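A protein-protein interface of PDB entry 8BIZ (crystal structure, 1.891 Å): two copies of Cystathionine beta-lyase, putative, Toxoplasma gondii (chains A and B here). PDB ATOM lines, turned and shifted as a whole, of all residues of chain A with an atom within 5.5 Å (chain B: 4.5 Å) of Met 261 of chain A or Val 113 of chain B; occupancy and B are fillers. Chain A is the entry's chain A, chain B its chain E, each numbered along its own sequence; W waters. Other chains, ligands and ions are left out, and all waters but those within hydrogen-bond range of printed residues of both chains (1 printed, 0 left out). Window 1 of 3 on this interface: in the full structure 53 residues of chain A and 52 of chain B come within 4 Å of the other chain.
The side-chain hydroxyl of Thr 114 of chain B sits at hydrogen-bond distance from the backbone carbonyl oxygen of Ala 110 of chain B, 2.7 Å away. O of Val 113 of chain B is in hydrogen-bond range of OG of Ser 117 of chain B (2.9 Å). O of Cys 139 of chain B is in hydrogen-bond range of N of Phe 144 of chain B, 3.2 Å away. O of Val 113 of chain A is in hydrogen-bond range of OG of Ser 117 of chain A (2.8 Å).
His 143 of chain B touches Ser 117 of chain A (CE1 to O, 3.5 Å). CD1 of Leu 257 of chain A touches ND1 of His 143 of chain B, at 3.7 Å. Met 109 of chain B touches Val 260 of chain A (CE to O, 3.4 Å). Val 260 of chain A touches Val 113 of chain B (O to CG1, 3.7 Å). Val 260 of chain A touches Cys 139 of chain B. O of Met 261 of chain A touches CA of Ala 110 of chain B (3.4 Å). Val 113 of chain B touches Met 261 of chain A. Ala 110 of chain B touches Gly 262 of chain A (CB to O, 3.4 Å).
Of chain B, only Ala 110 and Val 113 come within 4 Å of Met 261 of chain A. Val 113 of chain B touches just these residues of chain A: Val 260 and Met 261. Printed residues of chain B within 4 Å of Val 260 of chain A: Met 109 (3.4 Å), Val 113 (3.7 Å) and Cys 139 (3.4 Å). Printed residues of chain A within 4 Å of Met 109 of chain B: Val 260. Of the printed residues of chain B, Leu 257 of chain A touches His 143 (3.7 Å). Of the printed residues of chain A, Ala 110 of chain B touches Met 261 and Gly 262. Of the printed residues of chain B, Gly 262 of chain A touches Ala 110 (3.4 Å).
Hydrophobic or aromatic side chains of chain A that line the printed part of chain B: Leu 257 and Val 260. Among the printed residues, 8 pairs touch across the chains. Among the printed residues, no Asp or Glu carboxylate lies within 4 Å of a Lys or Arg side-chain nitrogen of the other chain.
Positions printed for both chains: 113, 114 and 117.
Water W1 bridges OG of Ser 117 of chain A (2.8 Å) and NE2 of His 143 of chain B (2.9 Å).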
ATOM      1  N   VAL A 113       6.759 -11.723  10.154  1.00  0.00           N
ATOM      2  CA  VAL A 113       7.351 -10.621   9.405  1.00  0.00           C
ATOM      3  C   VAL A 113       8.050  -9.644  10.340  1.00  0.00           C
ATOM      4  O   VAL A 113       9.083  -9.068   9.987  1.00  0.00           O
ATOM      5  CB  VAL A 113       6.260  -9.944   8.552  1.00  0.00           C
ATOM      6  CG1 VAL A 113       6.609  -8.516   8.177  1.00  0.00           C
ATOM      7  CG2 VAL A 113       5.953 -10.809   7.339  1.00  0.00           C
ATOM      8  N   THR A 114       7.516  -9.441  11.546  1.00  0.00           N
ATOM      9  CA  THR A 114       8.190  -8.532  12.467  1.00  0.00           C
ATOM     10  C   THR A 114       9.521  -9.121  12.924  1.00  0.00           C
ATOM     11  O   THR A 114      10.498  -8.391  13.130  1.00  0.00           O
ATOM     12  CB  THR A 114       7.297  -8.207  13.670  1.00  0.00           C
ATOM     13  OG1 THR A 114       6.076  -7.628  13.211  1.00  0.00           O
ATOM     14  CG2 THR A 114       7.988  -7.230  14.605  1.00  0.00           C
ATOM     15  N   SER A 117      11.869  -8.602  10.062  1.00  0.00           N
ATOM     16  CA  SER A 117      12.190  -7.185   9.933  1.00  0.00           C
ATOM     17  C   SER A 117      13.161  -6.730  11.016  1.00  0.00           C
ATOM     18  O   SER A 117      13.992  -5.844  10.781  1.00  0.00           O
ATOM     19  CB  SER A 117      10.910  -6.349  10.001  1.00  0.00           C
ATOM     20  OG  SER A 117      10.039  -6.629   8.915  1.00  0.00           O
ATOM     21  N   PHE A 256       9.324  -2.409  20.222  1.00  0.00           N
ATOM     22  CA  PHE A 256       9.637  -1.184  19.493  1.00  0.00           C
ATOM     23  C   PHE A 256       9.217  -1.294  18.030  1.00  0.00           C
ATOM     24  O   PHE A 256       8.561  -0.391  17.474  1.00  0.00           O
ATOM     25  CB  PHE A 256      11.144  -0.915  19.603  1.00  0.00           C
ATOM     26  CG  PHE A 256      11.601   0.295  18.850  1.00  0.00           C
ATOM     27  CD1 PHE A 256      11.631   1.533  19.471  1.00  0.00           C
ATOM     28  CD2 PHE A 256      11.979   0.197  17.518  1.00  0.00           C
ATOM     29  CE1 PHE A 256      12.050   2.661  18.779  1.00  0.00           C
ATOM     30  CE2 PHE A 256      12.394   1.319  16.815  1.00  0.00           C
ATOM     31  CZ  PHE A 256      12.419   2.554  17.453  1.00  0.00           C
ATOM     32  N   LEU A 257       9.604  -2.394  17.372  1.00  0.00           N
ATOM     33  CA  LEU A 257       9.310  -2.481  15.946  1.00  0.00           C
ATOM     34  C   LEU A 257       7.822  -2.715  15.686  1.00  0.00           C
ATOM     35  O   LEU A 257       7.307  -2.291  14.643  1.00  0.00           O
ATOM     36  CB  LEU A 257      10.139  -3.580  15.287  1.00  0.00           C
ATOM     37  CG  LEU A 257      10.198  -3.464  13.763  1.00  0.00           C
ATOM     38  CD1 LEU A 257      10.770  -2.107  13.318  1.00  0.00           C
ATOM     39  CD2 LEU A 257      11.008  -4.594  13.161  1.00  0.00           C
ATOM     40  N   ARG A 258       7.116  -3.392  16.597  1.00  0.00           N
ATOM     41  CA  ARG A 258       5.666  -3.520  16.459  1.00  0.00           C
ATOM     42  C   ARG A 258       5.003  -2.149  16.440  1.00  0.00           C
ATOM     43  O   ARG A 258       4.079  -1.904  15.654  1.00  0.00           O
ATOM     44  CB  ARG A 258       5.083  -4.358  17.598  1.00  0.00           C
ATOM     45  CG  ARG A 258       3.578  -4.562  17.475  1.00  0.00           C
ATOM     46  CD  ARG A 258       3.004  -5.295  18.676  1.00  0.00           C
ATOM     47  NE  ARG A 258       3.034  -4.460  19.867  1.00  0.00           N
ATOM     48  CZ  ARG A 258       2.560  -4.840  21.044  1.00  0.00           C
ATOM     49  NH1 ARG A 258       2.030  -6.045  21.175  1.00  0.00           N
ATOM     50  NH2 ARG A 258       2.626  -4.029  22.088  1.00  0.00           N
ATOM     51  N   ASN A 259       5.449  -1.247  17.326  1.00  0.00           N
ATOM     52  CA  ASN A 259       4.901   0.112  17.308  1.00  0.00           C
ATOM     53  C   ASN A 259       5.200   0.806  15.981  1.00  0.00           C
ATOM     54  O   ASN A 259       4.378   1.576  15.475  1.00  0.00           O
ATOM     55  CB  ASN A 259       5.468   0.947  18.456  1.00  0.00           C
ATOM     56  CG  ASN A 259       4.817   2.317  18.550  1.00  0.00           C
ATOM     57  OD1 ASN A 259       3.599   2.446  18.436  1.00  0.00           O
ATOM     58  ND2 ASN A 259       5.635   3.357  18.703  1.00  0.00           N
ATOM     59  N   VAL A 260       6.387   0.577  15.420  1.00  0.00           N
ATOM     60  CA  VAL A 260       6.725   1.224  14.148  1.00  0.00           C
ATOM     61  C   VAL A 260       5.894   0.651  13.000  1.00  0.00           C
ATOM     62  O   VAL A 260       5.435   1.388  12.119  1.00  0.00           O
ATOM     63  CB  VAL A 260       8.238   1.117  13.874  1.00  0.00           C
ATOM     64  CG1 VAL A 260       8.569   1.558  12.469  1.00  0.00           C
ATOM     65  CG2 VAL A 260       8.995   1.959  14.881  1.00  0.00           C
ATOM     66  N   MET A 261       5.690  -0.665  12.979  1.00  0.00           N
ATOM     67  CA  MET A 261       5.030  -1.296  11.847  1.00  0.00           C
ATOM     68  C   MET A 261       3.504  -1.272  11.947  1.00  0.00           C
ATOM     69  O   MET A 261       2.832  -1.597  10.961  1.00  0.00           O
ATOM     70  CB  MET A 261       5.546  -2.717  11.724  1.00  0.00           C
ATOM     71  CG  MET A 261       7.046  -2.696  11.475  1.00  0.00           C
ATOM     72  SD  MET A 261       7.607  -4.258  10.827  1.00  0.00           S
ATOM     73  CE  MET A 261       7.360  -3.974   9.076  1.00  0.00           C
ATOM     74  N   GLY A 262       2.956  -0.894  13.100  1.00  0.00           N
ATOM     75  CA  GLY A 262       1.516  -0.711  13.253  1.00  0.00           C
ATOM     76  C   GLY A 262       0.710  -1.980  13.096  1.00  0.00           C
ATOM     77  O   GLY A 262      -0.401  -1.933  12.561  1.00  0.00           O
ATOM     78  N   ASN A 263       1.235  -3.118  13.565  1.00  0.00           N
ATOM     79  CA  ASN A 263       0.580  -4.405  13.342  1.00  0.00           C
ATOM     80  C   ASN A 263       0.162  -5.076  14.656  1.00  0.00           C
ATOM     81  O   ASN A 263      -0.007  -6.296  14.708  1.00  0.00           O
ATOM     82  CB  ASN A 263       1.482  -5.310  12.497  1.00  0.00           C
ATOM     83  CG  ASN A 263       2.877  -5.495  13.092  1.00  0.00           C
ATOM     84  OD1 ASN A 263       3.179  -5.004  14.179  1.00  0.00           O
ATOM     85  ND2 ASN A 263       3.762  -6.137  12.326  1.00  0.00           N
ATOM     86  N   MET B 109      -0.149   3.471  10.451  1.00  0.00           N
ATOM     87  CA  MET B 109       1.268   3.151  10.278  1.00  0.00           C
ATOM     88  C   MET B 109       1.449   1.886   9.440  1.00  0.00           C
ATOM     89  O   MET B 109       2.415   1.774   8.677  1.00  0.00           O
ATOM     90  CB  MET B 109       1.954   2.978  11.636  1.00  0.00           C
ATOM     91  CG  MET B 109       2.305   4.304  12.352  1.00  0.00           C
ATOM     92  SD  MET B 109       3.234   5.470  11.333  1.00  0.00           S
ATOM     93  CE  MET B 109       4.623   4.446  10.849  1.00  0.00           C
ATOM     94  N   ALA B 110       0.546   0.910   9.577  1.00  0.00           N
ATOM     95  CA  ALA B 110       0.643  -0.291   8.744  1.00  0.00           C
ATOM     96  C   ALA B 110       0.433   0.040   7.265  1.00  0.00           C
ATOM     97  O   ALA B 110       1.125  -0.500   6.393  1.00  0.00           O
ATOM     98  CB  ALA B 110      -0.365  -1.336   9.208  1.00  0.00           C
ATOM     99  N   ALA B 111      -0.514   0.930   6.959  1.00  0.00           N
ATOM    100  CA  ALA B 111      -0.682   1.372   5.575  1.00  0.00           C
ATOM    101  C   ALA B 111       0.587   2.038   5.042  1.00  0.00           C
ATOM    102  O   ALA B 111       1.046   1.735   3.930  1.00  0.00           O
ATOM    103  CB  ALA B 111      -1.868   2.331   5.489  1.00  0.00           C
ATOM    104  N   THR B 112       1.177   2.940   5.836  1.00  0.00           N
ATOM    105  CA  THR B 112       2.387   3.649   5.415  1.00  0.00           C
ATOM    106  C   THR B 112       3.554   2.688   5.204  1.00  0.00           C
ATOM    107  O   THR B 112       4.273   2.765   4.191  1.00  0.00           O
ATOM    108  CB  THR B 112       2.772   4.701   6.460  1.00  0.00           C
ATOM    109  OG1 THR B 112       1.694   5.629   6.625  1.00  0.00           O
ATOM    110  CG2 THR B 112       4.065   5.427   6.067  1.00  0.00           C
ATOM    111  N   VAL B 113       3.785   1.790   6.168  1.00  0.00           N
ATOM    112  CA  VAL B 113       4.922   0.891   6.023  1.00  0.00           C
ATOM    113  C   VAL B 113       4.672  -0.108   4.901  1.00  0.00           C
ATOM    114  O   VAL B 113       5.624  -0.586   4.285  1.00  0.00           O
ATOM    115  CB  VAL B 113       5.272   0.172   7.343  1.00  0.00           C
ATOM    116  CG1 VAL B 113       5.502   1.173   8.455  1.00  0.00           C
ATOM    117  CG2 VAL B 113       4.238  -0.867   7.705  1.00  0.00           C
ATOM    118  N   THR B 114       3.409  -0.421   4.585  1.00  0.00           N
ATOM    119  CA  THR B 114       3.165  -1.261   3.417  1.00  0.00           C
ATOM    120  C   THR B 114       3.526  -0.520   2.133  1.00  0.00           C
ATOM    121  O   THR B 114       4.061  -1.125   1.199  1.00  0.00           O
ATOM    122  CB  THR B 114       1.708  -1.744   3.371  1.00  0.00           C
ATOM    123  OG1 THR B 114       1.404  -2.435   4.582  1.00  0.00           O
ATOM    124  CG2 THR B 114       1.502  -2.697   2.194  1.00  0.00           C
ATOM    125  N   ILE B 115       3.262   0.788   2.064  1.00  0.00           N
ATOM    126  CA  ILE B 115       3.726   1.565   0.909  1.00  0.00           C
ATOM    127  C   ILE B 115       5.249   1.484   0.791  1.00  0.00           C
ATOM    128  O   ILE B 115       5.797   1.170  -0.279  1.00  0.00           O
ATOM    129  CB  ILE B 115       3.247   3.028   0.996  1.00  0.00           C
ATOM    130  CG1 ILE B 115       1.727   3.090   0.942  1.00  0.00           C
ATOM    131  CG2 ILE B 115       3.883   3.872  -0.117  1.00  0.00           C
ATOM    132  CD1 ILE B 115       1.171   2.429  -0.273  1.00  0.00           C
ATOM    133  N   PHE B 116       5.956   1.786   1.882  1.00  0.00           N
ATOM    134  CA  PHE B 116       7.421   1.740   1.832  1.00  0.00           C
ATOM    135  C   PHE B 116       7.928   0.333   1.487  1.00  0.00           C
ATOM    136  O   PHE B 116       8.898   0.184   0.728  1.00  0.00           O
ATOM    137  CB  PHE B 116       8.021   2.220   3.158  1.00  0.00           C
ATOM    138  CG  PHE B 116       7.861   3.699   3.415  1.00  0.00           C
ATOM    139  CD1 PHE B 116       7.800   4.610   2.371  1.00  0.00           C
ATOM    140  CD2 PHE B 116       7.831   4.181   4.712  1.00  0.00           C
ATOM    141  CE1 PHE B 116       7.678   5.986   2.628  1.00  0.00           C
ATOM    142  CE2 PHE B 116       7.707   5.545   4.973  1.00  0.00           C
ATOM    143  CZ  PHE B 116       7.628   6.442   3.938  1.00  0.00           C
ATOM    144  N   SER B 117       7.278  -0.711   2.017  1.00  0.00           N
ATOM    145  CA  SER B 117       7.701  -2.085   1.745  1.00  0.00           C
ATOM    146  C   SER B 117       7.486  -2.471   0.285  1.00  0.00           C
ATOM    147  O   SER B 117       8.297  -3.209  -0.295  1.00  0.00           O
ATOM    148  CB  SER B 117       6.939  -3.063   2.643  1.00  0.00           C
ATOM    149  OG  SER B 117       7.307  -2.934   4.005  1.00  0.00           O
ATOM    150  N   CYS B 139       9.765   5.699  11.037  1.00  0.00           N
ATOM    151  CA  CYS B 139       9.828   4.401  10.369  1.00  0.00           C
ATOM    152  C   CYS B 139      10.710   4.483   9.128  1.00  0.00           C
ATOM    153  O   CYS B 139      11.313   3.484   8.729  1.00  0.00           O
ATOM    154  CB  CYS B 139       8.443   3.882   9.982  1.00  0.00           C
ATOM    155  SG  CYS B 139       7.807   4.479   8.390  1.00  0.00           S
ATOM    156  N   HIS B 143      14.129   2.471  10.430  1.00  0.00           N
ATOM    157  CA  HIS B 143      13.921   1.100   9.985  1.00  0.00           C
ATOM    158  C   HIS B 143      14.285   0.876   8.527  1.00  0.00           C
ATOM    159  O   HIS B 143      15.235   0.144   8.234  1.00  0.00           O
ATOM    160  CB  HIS B 143      12.476   0.660  10.210  1.00  0.00           C
ATOM    161  CG  HIS B 143      12.222  -0.742   9.763  1.00  0.00           C
ATOM    162  ND1 HIS B 143      12.921  -1.819  10.262  1.00  0.00           N
ATOM    163  CD2 HIS B 143      11.407  -1.235   8.801  1.00  0.00           C
ATOM    164  CE1 HIS B 143      12.520  -2.921   9.654  1.00  0.00           C
ATOM    165  NE2 HIS B 143      11.601  -2.594   8.763  1.00  0.00           N
ATOM    166  N   PHE B 144      13.526   1.472   7.606  1.00  0.00           N
ATOM    167  CA  PHE B 144      13.732   1.171   6.195  1.00  0.00           C
ATOM    168  C   PHE B 144      15.098   1.632   5.704  1.00  0.00           C
ATOM    169  O   PHE B 144      15.626   1.054   4.749  1.00  0.00           O
ATOM    170  CB  PHE B 144      12.614   1.785   5.350  1.00  0.00           C
ATOM    171  CG  PHE B 144      11.339   0.994   5.405  1.00  0.00           C
ATOM    172  CD1 PHE B 144      11.188  -0.164   4.655  1.00  0.00           C
ATOM    173  CD2 PHE B 144      10.316   1.377   6.253  1.00  0.00           C
ATOM    174  CE1 PHE B 144      10.023  -0.907   4.727  1.00  0.00           C
ATOM    175  CE2 PHE B 144       9.148   0.637   6.336  1.00  0.00           C
ATOM    176  CZ  PHE B 144       9.001  -0.505   5.575  1.00  0.00           C
HETATM  177  O   HOH W   1      10.413  -4.621   7.054  1.00  0.00           O
